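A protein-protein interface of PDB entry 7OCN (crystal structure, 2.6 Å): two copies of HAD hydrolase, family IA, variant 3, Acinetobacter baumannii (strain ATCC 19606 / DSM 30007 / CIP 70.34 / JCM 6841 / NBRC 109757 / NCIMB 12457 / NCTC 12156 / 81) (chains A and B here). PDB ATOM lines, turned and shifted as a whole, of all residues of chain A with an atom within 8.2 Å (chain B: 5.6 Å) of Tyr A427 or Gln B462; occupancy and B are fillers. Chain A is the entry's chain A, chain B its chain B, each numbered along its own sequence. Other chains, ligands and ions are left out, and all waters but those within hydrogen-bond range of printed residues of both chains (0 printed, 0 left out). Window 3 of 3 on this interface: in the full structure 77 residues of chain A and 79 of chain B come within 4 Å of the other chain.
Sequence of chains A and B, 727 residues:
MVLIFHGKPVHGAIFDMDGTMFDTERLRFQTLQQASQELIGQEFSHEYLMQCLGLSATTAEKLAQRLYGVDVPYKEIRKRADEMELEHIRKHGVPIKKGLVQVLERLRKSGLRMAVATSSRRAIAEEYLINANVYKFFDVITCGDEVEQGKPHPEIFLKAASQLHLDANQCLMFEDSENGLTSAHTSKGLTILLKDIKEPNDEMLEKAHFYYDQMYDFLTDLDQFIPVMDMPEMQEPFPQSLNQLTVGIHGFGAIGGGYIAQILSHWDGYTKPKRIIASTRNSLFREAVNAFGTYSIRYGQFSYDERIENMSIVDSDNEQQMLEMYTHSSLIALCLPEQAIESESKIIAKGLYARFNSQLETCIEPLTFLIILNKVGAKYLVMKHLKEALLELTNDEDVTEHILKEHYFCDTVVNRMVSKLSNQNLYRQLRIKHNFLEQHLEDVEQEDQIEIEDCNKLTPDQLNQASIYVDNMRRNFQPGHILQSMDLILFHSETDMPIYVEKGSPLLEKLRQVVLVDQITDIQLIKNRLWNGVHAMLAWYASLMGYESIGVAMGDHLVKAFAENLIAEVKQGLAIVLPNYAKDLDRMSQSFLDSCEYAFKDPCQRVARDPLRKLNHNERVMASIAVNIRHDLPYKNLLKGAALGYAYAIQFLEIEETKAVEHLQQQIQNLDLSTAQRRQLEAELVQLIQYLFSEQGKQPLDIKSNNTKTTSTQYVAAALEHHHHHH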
ATOM      1  N   LEU A 284      -8.661 -34.234 -33.877  1.00  0.00           N
ATOM      2  CA  LEU A 284      -8.737 -33.301 -32.718  1.00  0.00           C
ATOM      3  C   LEU A 284      -9.798 -32.229 -32.996  1.00  0.00           C
ATOM      4  O   LEU A 284     -10.618 -31.968 -32.095  1.00  0.00           O
ATOM      5  CB  LEU A 284      -7.358 -32.672 -32.484  1.00  0.00           C
ATOM      6  CG  LEU A 284      -7.230 -31.796 -31.237  1.00  0.00           C
ATOM      7  CD1 LEU A 284      -7.447 -32.610 -29.970  1.00  0.00           C
ATOM      8  CD2 LEU A 284      -5.875 -31.106 -31.200  1.00  0.00           C
ATOM      9  N   PHE A 285      -9.775 -31.639 -34.195  1.00  0.00           N
ATOM     10  CA  PHE A 285     -10.749 -30.617 -34.668  1.00  0.00           C
ATOM     11  C   PHE A 285     -12.162 -31.216 -34.697  1.00  0.00           C
ATOM     12  O   PHE A 285     -13.095 -30.558 -34.200  1.00  0.00           O
ATOM     13  CB  PHE A 285     -10.357 -30.081 -36.049  1.00  0.00           C
ATOM     14  CG  PHE A 285      -9.565 -28.798 -36.027  1.00  0.00           C
ATOM     15  CD1 PHE A 285      -8.297 -28.753 -35.467  1.00  0.00           C
ATOM     16  CD2 PHE A 285     -10.086 -27.634 -36.571  1.00  0.00           C
ATOM     17  CE1 PHE A 285      -7.570 -27.572 -35.448  1.00  0.00           C
ATOM     18  CE2 PHE A 285      -9.359 -26.453 -36.551  1.00  0.00           C
ATOM     19  CZ  PHE A 285      -8.103 -26.424 -35.990  1.00  0.00           C
ATOM     20  N   ALA A 288     -13.578 -32.213 -31.071  1.00  0.00           N
ATOM     21  CA  ALA A 288     -13.680 -30.961 -30.279  1.00  0.00           C
ATOM     22  C   ALA A 288     -14.968 -30.211 -30.640  1.00  0.00           C
ATOM     23  O   ALA A 288     -15.703 -29.822 -29.710  1.00  0.00           O
ATOM     24  CB  ALA A 288     -12.463 -30.097 -30.510  1.00  0.00           C
ATOM     25  N   LEU A 421      -6.086 -22.504 -36.612  1.00  0.00           N
ATOM     26  CA  LEU A 421      -5.370 -22.610 -35.312  1.00  0.00           C
ATOM     27  C   LEU A 421      -4.594 -23.933 -35.273  1.00  0.00           C
ATOM     28  O   LEU A 421      -5.111 -24.937 -35.802  1.00  0.00           O
ATOM     29  CB  LEU A 421      -6.383 -22.524 -34.164  1.00  0.00           C
ATOM     30  CG  LEU A 421      -5.787 -22.274 -32.779  1.00  0.00           C
ATOM     31  CD1 LEU A 421      -5.243 -20.857 -32.669  1.00  0.00           C
ATOM     32  CD2 LEU A 421      -6.817 -22.533 -31.690  1.00  0.00           C
ATOM     33  N   SER A 422      -3.398 -23.925 -34.676  1.00  0.00           N
ATOM     34  CA  SER A 422      -2.498 -25.104 -34.563  1.00  0.00           C
ATOM     35  C   SER A 422      -3.066 -26.091 -33.536  1.00  0.00           C
ATOM     36  O   SER A 422      -3.850 -25.658 -32.668  1.00  0.00           O
ATOM     37  CB  SER A 422      -1.093 -24.689 -34.211  1.00  0.00           C
ATOM     38  OG  SER A 422      -1.036 -24.152 -32.898  1.00  0.00           O
ATOM     39  N   ASN A 423      -2.678 -27.365 -33.643  1.00  0.00           N
ATOM     40  CA  ASN A 423      -3.123 -28.463 -32.742  1.00  0.00           C
ATOM     41  C   ASN A 423      -2.561 -28.235 -31.333  1.00  0.00           C
ATOM     42  O   ASN A 423      -3.254 -28.603 -30.364  1.00  0.00           O
ATOM     43  CB  ASN A 423      -2.732 -29.838 -33.291  1.00  0.00           C
ATOM     44  CG  ASN A 423      -3.522 -30.221 -34.525  1.00  0.00           C
ATOM     45  OD1 ASN A 423      -3.864 -29.366 -35.341  1.00  0.00           O
ATOM     46  ND2 ASN A 423      -3.819 -31.500 -34.670  1.00  0.00           N
ATOM     47  N   GLN A 424      -1.358 -27.656 -31.226  1.00  0.00           N
ATOM     48  CA  GLN A 424      -0.721 -27.276 -29.934  1.00  0.00           C
ATOM     49  C   GLN A 424      -1.569 -26.196 -29.251  1.00  0.00           C
ATOM     50  O   GLN A 424      -1.867 -26.357 -28.051  1.00  0.00           O
ATOM     51  CB  GLN A 424       0.716 -26.792 -30.149  1.00  0.00           C
ATOM     52  CG  GLN A 424       1.708 -27.918 -30.414  1.00  0.00           C
ATOM     53  CD  GLN A 424       3.144 -27.464 -30.310  1.00  0.00           C
ATOM     54  OE1 GLN A 424       3.461 -26.288 -30.478  1.00  0.00           O
ATOM     55  NE2 GLN A 424       4.032 -28.404 -30.030  1.00  0.00           N
ATOM     56  N   ASN A 425      -1.941 -25.145 -29.991  1.00  0.00           N
ATOM     57  CA  ASN A 425      -2.758 -24.006 -29.490  1.00  0.00           C
ATOM     58  C   ASN A 425      -4.171 -24.491 -29.142  1.00  0.00           C
ATOM     59  O   ASN A 425      -4.747 -23.959 -28.175  1.00  0.00           O
ATOM     60  CB  ASN A 425      -2.812 -22.849 -30.493  1.00  0.00           C
ATOM     61  CG  ASN A 425      -1.526 -22.052 -30.563  1.00  0.00           C
ATOM     62  OD1 ASN A 425      -0.796 -21.949 -29.580  1.00  0.00           O
ATOM     63  ND2 ASN A 425      -1.244 -21.475 -31.718  1.00  0.00           N
ATOM     64  N   LEU A 426      -4.706 -25.454 -29.902  1.00  0.00           N
ATOM     65  CA  LEU A 426      -6.053 -26.043 -29.669  1.00  0.00           C
ATOM     66  C   LEU A 426      -6.035 -26.837 -28.359  1.00  0.00           C
ATOM     67  O   LEU A 426      -6.942 -26.622 -27.533  1.00  0.00           O
ATOM     68  CB  LEU A 426      -6.443 -26.931 -30.856  1.00  0.00           C
ATOM     69  CG  LEU A 426      -7.789 -27.647 -30.734  1.00  0.00           C
ATOM     70  CD1 LEU A 426      -8.898 -26.679 -30.348  1.00  0.00           C
ATOM     71  CD2 LEU A 426      -8.139 -28.363 -32.029  1.00  0.00           C
ATOM     72  N   TYR A 427      -5.041 -27.713 -28.179  1.00  0.00           N
ATOM     73  CA  TYR A 427      -4.834 -28.525 -26.950  1.00  0.00           C
ATOM     74  C   TYR A 427      -4.777 -27.594 -25.733  1.00  0.00           C
ATOM     75  O   TYR A 427      -5.472 -27.872 -24.735  1.00  0.00           O
ATOM     76  CB  TYR A 427      -3.563 -29.374 -27.059  1.00  0.00           C
ATOM     77  CG  TYR A 427      -3.231 -30.153 -25.811  1.00  0.00           C
ATOM     78  CD1 TYR A 427      -4.013 -31.224 -25.409  1.00  0.00           C
ATOM     79  CD2 TYR A 427      -2.141 -29.815 -25.024  1.00  0.00           C
ATOM     80  CE1 TYR A 427      -3.721 -31.942 -24.260  1.00  0.00           C
ATOM     81  CE2 TYR A 427      -1.833 -30.525 -23.873  1.00  0.00           C
ATOM     82  CZ  TYR A 427      -2.626 -31.592 -23.490  1.00  0.00           C
ATOM     83  OH  TYR A 427      -2.332 -32.296 -22.358  1.00  0.00           O
ATOM     84  N   ARG A 428      -3.978 -26.525 -25.827  1.00  0.00           N
ATOM     85  CA  ARG A 428      -3.841 -25.469 -24.787  1.00  0.00           C
ATOM     86  C   ARG A 428      -5.232 -24.925 -24.434  1.00  0.00           C
ATOM     87  O   ARG A 428      -5.535 -24.814 -23.231  1.00  0.00           O
ATOM     88  CB  ARG A 428      -2.939 -24.330 -25.278  1.00  0.00           C
ATOM     89  CG  ARG A 428      -2.578 -23.310 -24.207  1.00  0.00           C
ATOM     90  CD  ARG A 428      -2.919 -21.889 -24.618  1.00  0.00           C
ATOM     91  NE  ARG A 428      -2.158 -21.433 -25.775  1.00  0.00           N
ATOM     92  CZ  ARG A 428      -0.930 -20.918 -25.736  1.00  0.00           C
ATOM     93  NH1 ARG A 428      -0.344 -20.533 -26.858  1.00  0.00           N
ATOM     94  NH2 ARG A 428      -0.285 -20.790 -24.588  1.00  0.00           N
ATOM     95  N   GLN A 429      -6.035 -24.603 -25.452  1.00  0.00           N
ATOM     96  CA  GLN A 429      -7.403 -24.038 -25.297  1.00  0.00           C
ATOM     97  C   GLN A 429      -8.321 -25.094 -24.668  1.00  0.00           C
ATOM     98  O   GLN A 429      -9.055 -24.740 -23.726  1.00  0.00           O
ATOM     99  CB  GLN A 429      -7.943 -23.560 -26.646  1.00  0.00           C
ATOM    100  CG  GLN A 429      -9.176 -22.676 -26.526  1.00  0.00           C
ATOM    101  CD  GLN A 429      -9.738 -22.266 -27.866  1.00  0.00           C
ATOM    102  OE1 GLN A 429     -10.947 -22.287 -28.081  1.00  0.00           O
ATOM    103  NE2 GLN A 429      -8.860 -21.890 -28.782  1.00  0.00           N
ATOM    104  N   LEU A 430      -8.269 -26.336 -25.162  1.00  0.00           N
ATOM    105  CA  LEU A 430      -9.093 -27.477 -24.670  1.00  0.00           C
ATOM    106  C   LEU A 430      -8.763 -27.771 -23.202  1.00  0.00           C
ATOM    107  O   LEU A 430      -9.676 -28.210 -22.476  1.00  0.00           O
ATOM    108  CB  LEU A 430      -8.841 -28.712 -25.545  1.00  0.00           C
ATOM    109  CG  LEU A 430      -9.435 -28.663 -26.953  1.00  0.00           C
ATOM    110  CD1 LEU A 430      -8.861 -29.773 -27.820  1.00  0.00           C
ATOM    111  CD2 LEU A 430     -10.953 -28.753 -26.914  1.00  0.00           C
ATOM    112  N   ARG A 431      -7.513 -27.544 -22.784  1.00  0.00           N
ATOM    113  CA  ARG A 431      -7.039 -27.769 -21.391  1.00  0.00           C
ATOM    114  C   ARG A 431      -7.622 -26.690 -20.469  1.00  0.00           C
ATOM    115  O   ARG A 431      -8.148 -27.053 -19.399  1.00  0.00           O
ATOM    116  CB  ARG A 431      -5.506 -27.773 -21.344  1.00  0.00           C
ATOM    117  CG  ARG A 431      -4.924 -28.079 -19.972  1.00  0.00           C
ATOM    118  CD  ARG A 431      -3.425 -28.318 -20.014  1.00  0.00           C
ATOM    119  NE  ARG A 431      -2.715 -27.335 -20.825  1.00  0.00           N
ATOM    120  CZ  ARG A 431      -2.478 -26.073 -20.473  1.00  0.00           C
ATOM    121  NH1 ARG A 431      -2.898 -25.607 -19.308  1.00  0.00           N
ATOM    122  NH2 ARG A 431      -1.820 -25.274 -21.297  1.00  0.00           N
ATOM    123  N   ILE A 432      -7.529 -25.418 -20.872  1.00  0.00           N
ATOM    124  CA  ILE A 432      -7.973 -24.236 -20.071  1.00  0.00           C
ATOM    125  C   ILE A 432      -9.509 -24.213 -20.009  1.00  0.00           C
ATOM    126  O   ILE A 432     -10.042 -23.822 -18.953  1.00  0.00           O
ATOM    127  CB  ILE A 432      -7.387 -22.927 -20.641  1.00  0.00           C
ATOM    128  CG1 ILE A 432      -5.860 -22.894 -20.512  1.00  0.00           C
ATOM    129  CG2 ILE A 432      -8.027 -21.710 -19.989  1.00  0.00           C
ATOM    130  CD1 ILE A 432      -5.186 -21.849 -21.371  1.00  0.00           C
ATOM    131  N   LYS A 433     -10.188 -24.610 -21.091  1.00  0.00           N
ATOM    132  CA  LYS A 433     -11.675 -24.667 -21.169  1.00  0.00           C
ATOM    133  C   LYS A 433     -12.193 -25.801 -20.272  1.00  0.00           C
ATOM    134  O   LYS A 433     -13.174 -25.563 -19.542  1.00  0.00           O
ATOM    135  CB  LYS A 433     -12.150 -24.831 -22.618  1.00  0.00           C
ATOM    136  CG  LYS A 433     -12.500 -23.533 -23.338  1.00  0.00           C
ATOM    137  CD  LYS A 433     -11.396 -22.493 -23.336  1.00  0.00           C
ATOM    138  CE  LYS A 433     -11.848 -21.150 -23.871  1.00  0.00           C
ATOM    139  NZ  LYS A 433     -12.310 -21.241 -25.278  1.00  0.00           N
ATOM    140  N   HIS A 434     -11.561 -26.979 -20.328  1.00  0.00           N
ATOM    141  CA  HIS A 434     -11.892 -28.166 -19.490  1.00  0.00           C
ATOM    142  C   HIS A 434     -11.761 -27.805 -18.004  1.00  0.00           C
ATOM    143  O   HIS A 434     -12.548 -28.337 -17.198  1.00  0.00           O
ATOM    144  CB  HIS A 434     -11.007 -29.364 -19.860  1.00  0.00           C
ATOM    145  CG  HIS A 434     -11.216 -30.560 -18.990  1.00  0.00           C
ATOM    146  ND1 HIS A 434     -10.482 -30.773 -17.838  1.00  0.00           N
ATOM    147  CD2 HIS A 434     -12.067 -31.601 -19.094  1.00  0.00           C
ATOM    148  CE1 HIS A 434     -10.875 -31.895 -17.271  1.00  0.00           C
ATOM    149  NE2 HIS A 434     -11.845 -32.423 -18.022  1.00  0.00           N
ATOM    150  N   LEU A 488     -15.274 -21.897 -28.538  1.00  0.00           N
ATOM    151  CA  LEU A 488     -14.193 -22.778 -29.055  1.00  0.00           C
ATOM    152  C   LEU A 488     -13.613 -22.144 -30.326  1.00  0.00           C
ATOM    153  O   LEU A 488     -14.151 -22.406 -31.420  1.00  0.00           O
ATOM    154  CB  LEU A 488     -14.764 -24.175 -29.323  1.00  0.00           C
ATOM    155  CG  LEU A 488     -13.749 -25.240 -29.735  1.00  0.00           C
ATOM    156  CD1 LEU A 488     -12.827 -25.594 -28.578  1.00  0.00           C
ATOM    157  CD2 LEU A 488     -14.452 -26.486 -30.251  1.00  0.00           C
ATOM    158  N   LEU A 490     -11.260 -21.668 -33.368  1.00  0.00           N
ATOM    159  CA  LEU A 490     -10.484 -22.558 -34.276  1.00  0.00           C
ATOM    160  C   LEU A 490      -9.906 -21.775 -35.463  1.00  0.00           C
ATOM    161  O   LEU A 490      -9.064 -22.359 -36.175  1.00  0.00           O
ATOM    162  CB  LEU A 490     -11.398 -23.685 -34.766  1.00  0.00           C
ATOM    163  CG  LEU A 490     -11.931 -24.627 -33.687  1.00  0.00           C
ATOM    164  CD1 LEU A 490     -12.843 -25.678 -34.297  1.00  0.00           C
ATOM    165  CD2 LEU A 490     -10.796 -25.292 -32.922  1.00  0.00           C
ATOM    166  N   LEU B 458       1.205 -33.750 -32.331  1.00  0.00           N
ATOM    167  CA  LEU B 458       1.134 -33.784 -30.842  1.00  0.00           C
ATOM    168  C   LEU B 458       1.725 -35.104 -30.334  1.00  0.00           C
ATOM    169  O   LEU B 458       1.650 -36.110 -31.070  1.00  0.00           O
ATOM    170  CB  LEU B 458      -0.324 -33.632 -30.395  1.00  0.00           C
ATOM    171  CG  LEU B 458      -0.898 -32.217 -30.456  1.00  0.00           C
ATOM    172  CD1 LEU B 458      -2.402 -32.234 -30.228  1.00  0.00           C
ATOM    173  CD2 LEU B 458      -0.221 -31.304 -29.445  1.00  0.00           C
ATOM    174  N   THR B 459       2.280 -35.090 -29.117  1.00  0.00           N
ATOM    175  CA  THR B 459       2.912 -36.261 -28.452  1.00  0.00           C
ATOM    176  C   THR B 459       1.828 -37.251 -28.031  1.00  0.00           C
ATOM    177  O   THR B 459       0.688 -36.855 -27.796  1.00  0.00           O
ATOM    178  CB  THR B 459       3.761 -35.827 -27.249  1.00  0.00           C
ATOM    179  OG1 THR B 459       2.923 -35.107 -26.344  1.00  0.00           O
ATOM    180  CG2 THR B 459       4.944 -34.970 -27.642  1.00  0.00           C
ATOM    181  N   PRO B 460       2.141 -38.566 -27.934  1.00  0.00           N
ATOM    182  CA  PRO B 460       1.186 -39.558 -27.433  1.00  0.00           C
ATOM    183  C   PRO B 460       0.605 -39.220 -26.049  1.00  0.00           C
ATOM    184  O   PRO B 460      -0.544 -39.546 -25.813  1.00  0.00           O
ATOM    185  CB  PRO B 460       2.014 -40.851 -27.351  1.00  0.00           C
ATOM    186  CG  PRO B 460       3.109 -40.656 -28.376  1.00  0.00           C
ATOM    187  CD  PRO B 460       3.421 -39.175 -28.333  1.00  0.00           C
ATOM    188  N   ASP B 461       1.407 -38.589 -25.181  1.00  0.00           N
ATOM    189  CA  ASP B 461       1.018 -38.176 -23.804  1.00  0.00           C
ATOM    190  C   ASP B 461      -0.096 -37.125 -23.880  1.00  0.00           C
ATOM    191  O   ASP B 461      -1.117 -37.297 -23.182  1.00  0.00           O
ATOM    192  CB  ASP B 461       2.220 -37.640 -23.022  1.00  0.00           C
ATOM    193  CG  ASP B 461       3.276 -38.688 -22.711  1.00  0.00           C
ATOM    194  OD1 ASP B 461       3.263 -39.748 -23.369  1.00  0.00           O
ATOM    195  OD2 ASP B 461       4.102 -38.434 -21.812  1.00  0.00           O
ATOM    196  N   GLN B 462       0.104 -36.079 -24.689  1.00  0.00           N
ATOM    197  CA  GLN B 462      -0.861 -34.959 -24.888  1.00  0.00           C
ATOM    198  C   GLN B 462      -2.121 -35.482 -25.588  1.00  0.00           C
ATOM    199  O   GLN B 462      -3.230 -35.147 -25.128  1.00  0.00           O
ATOM    200  CB  GLN B 462      -0.219 -33.830 -25.698  1.00  0.00           C
ATOM    201  CG  GLN B 462       0.797 -33.017 -24.910  1.00  0.00           C
ATOM    202  CD  GLN B 462       1.396 -31.896 -25.725  1.00  0.00           C
ATOM    203  OE1 GLN B 462       1.752 -32.069 -26.889  1.00  0.00           O
ATOM    204  NE2 GLN B 462       1.517 -30.730 -25.111  1.00  0.00           N
ATOM    205  N   LEU B 463      -1.948 -36.268 -26.657  1.00  0.00           N
ATOM    206  CA  LEU B 463      -3.050 -36.865 -27.463  1.00  0.00           C
ATOM    207  C   LEU B 463      -3.938 -37.730 -26.559  1.00  0.00           C
ATOM    208  O   LEU B 463      -5.170 -37.705 -26.747  1.00  0.00           O
ATOM    209  CB  LEU B 463      -2.447 -37.693 -28.605  1.00  0.00           C
ATOM    210  CG  LEU B 463      -3.431 -38.164 -29.676  1.00  0.00           C
ATOM    211  CD1 LEU B 463      -3.938 -36.994 -30.504  1.00  0.00           C
ATOM    212  CD2 LEU B 463      -2.790 -39.211 -30.574  1.00  0.00           C
ATOM    213  N   ASN B 464      -3.329 -38.462 -25.619  1.00  0.00           N
ATOM    214  CA  ASN B 464      -4.025 -39.322 -24.624  1.00  0.00           C
ATOM    215  C   ASN B 464      -4.777 -38.434 -23.624  1.00  0.00           C
ATOM    216  O   ASN B 464      -5.922 -38.782 -23.275  1.00  0.00           O
ATOM    217  CB  ASN B 464      -3.047 -40.262 -23.912  1.00  0.00           C
ATOM    218  CG  ASN B 464      -3.726 -41.265 -23.003  1.00  0.00           C
ATOM    219  OD1 ASN B 464      -4.884 -41.619 -23.207  1.00  0.00           O
ATOM    220  ND2 ASN B 464      -3.006 -41.738 -21.998  1.00  0.00           N
ATOM    221  N   GLN B 465      -4.153 -37.335 -23.185  1.00  0.00           N
ATOM    222  CA  GLN B 465      -4.727 -36.363 -22.214  1.00  0.00           C
ATOM    223  C   GLN B 465      -5.874 -35.591 -22.879  1.00  0.00           C
ATOM    224  O   GLN B 465      -6.880 -35.324 -22.190  1.00  0.00           O
ATOM    225  CB  GLN B 465      -3.637 -35.412 -21.710  1.00  0.00           C
ATOM    226  CG  GLN B 465      -4.084 -34.508 -20.568  1.00  0.00           C
ATOM    227  CD  GLN B 465      -4.314 -35.252 -19.274  1.00  0.00           C
ATOM    228  OE1 GLN B 465      -3.566 -36.157 -18.911  1.00  0.00           O
ATOM    229  NE2 GLN B 465      -5.357 -34.862 -18.558  1.00  0.00           N
ATOM    230  N   ALA B 466      -5.721 -35.243 -24.162  1.00  0.00           N
ATOM    231  CA  ALA B 466      -6.724 -34.519 -24.981  1.00  0.00           C
ATOM    232  C   ALA B 466      -8.010 -35.349 -25.082  1.00  0.00           C
ATOM    233  O   ALA B 466      -9.101 -34.766 -24.930  1.00  0.00           O
ATOM    234  CB  ALA B 466      -6.158 -34.217 -26.347  1.00  0.00           C
ATOM    235  N   SER B 467      -7.876 -36.657 -25.330  1.00  0.00           N
ATOM    236  CA  SER B 467      -8.996 -37.631 -25.449  1.00  0.00           C
ATOM    237  C   SER B 467      -9.862 -37.596 -24.184  1.00  0.00           C
ATOM    238  O   SER B 467     -11.100 -37.601 -24.323  1.00  0.00           O
ATOM    239  CB  SER B 467      -8.481 -39.023 -25.718  1.00  0.00           C
ATOM    240  OG  SER B 467      -7.805 -39.083 -26.964  1.00  0.00           O
ATOM    241  N   TYR B 469     -10.146 -35.123 -21.911  1.00  0.00           N
ATOM    242  CA  TYR B 469     -10.778 -33.779 -21.814  1.00  0.00           C
ATOM    243  C   TYR B 469     -12.036 -33.728 -22.688  1.00  0.00           C
ATOM    244  O   TYR B 469     -13.103 -33.334 -22.177  1.00  0.00           O
ATOM    245  CB  TYR B 469      -9.804 -32.670 -22.232  1.00  0.00           C
ATOM    246  CG  TYR B 469      -8.624 -32.441 -21.319  1.00  0.00           C
ATOM    247  CD1 TYR B 469      -8.726 -32.587 -19.942  1.00  0.00           C
ATOM    248  CD2 TYR B 469      -7.403 -32.032 -21.832  1.00  0.00           C
ATOM    249  CE1 TYR B 469      -7.643 -32.361 -19.107  1.00  0.00           C
ATOM    250  CE2 TYR B 469      -6.312 -31.797 -21.011  1.00  0.00           C
ATOM    251  CZ  TYR B 469      -6.431 -31.963 -19.642  1.00  0.00           C
ATOM    252  OH  TYR B 469      -5.360 -31.738 -18.827  1.00  0.00           O
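No position is printed for both chains.
Of the 7 pairs that touch across the chains among the printed residues, none has its exchanged pair printed and touching as well.
Printed residues of chain B that touch a printed residue of chain A: Leu B458, Gln B462, Gln B465, Ala B466 and Tyr B469.
Of the printed residues of chain B, Leu A284 touches Leu B458 (3.8 Å).
Of the printed residues of chain B, Asn A423 touches Leu B458 (3.7 Å).
Gln A424 touches none of the printed residues of chain B.
Gln B462 touches one residue of chain A.
Of the printed residues of chain A, Ala B466 touches Tyr A427.
Printed residues of chain A within 4 Å of Tyr B469: Arg A431 and His A434.
The nearest residue of chain B that does not touch Tyr A427 is Tyr B469 (4.2 Å).
The nearest residue of chain A that does not touch Gln B462 is Gln A424 (5.3 Å).
The nearest printed residue of chain A that does not touch Gln B465 is Arg A431 (6.2 Å).
The side-chain hydroxyl (OG1) of Thr B459 sits at hydrogen-bond distance from the side-chain amide oxygen (OE1) of Gln B462.
The side-chain hydroxyl (OH) of Tyr B469 sits at hydrogen-bond distance from the side-chain amide nitrogen (NE2) of Gln B465 (3.1 Å).
CD1 of Leu B458 touches CD2 of Leu A284, 3.8 Å away.
Asn A423 touches Leu B458.
O of Gln B462 touches CE1 of Tyr A427 (3.4 Å).
OH of Tyr A427 touches CG of Gln B465, 3.3 Å away.
CD1 of Tyr A427 touches CB of Ala B466 (3.8 Å).
CG of Arg A431 touches OH of Tyr B469, at 3.9 Å.
His A434 touches Tyr B469 (ND1 to CD1, 3.3 Å).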
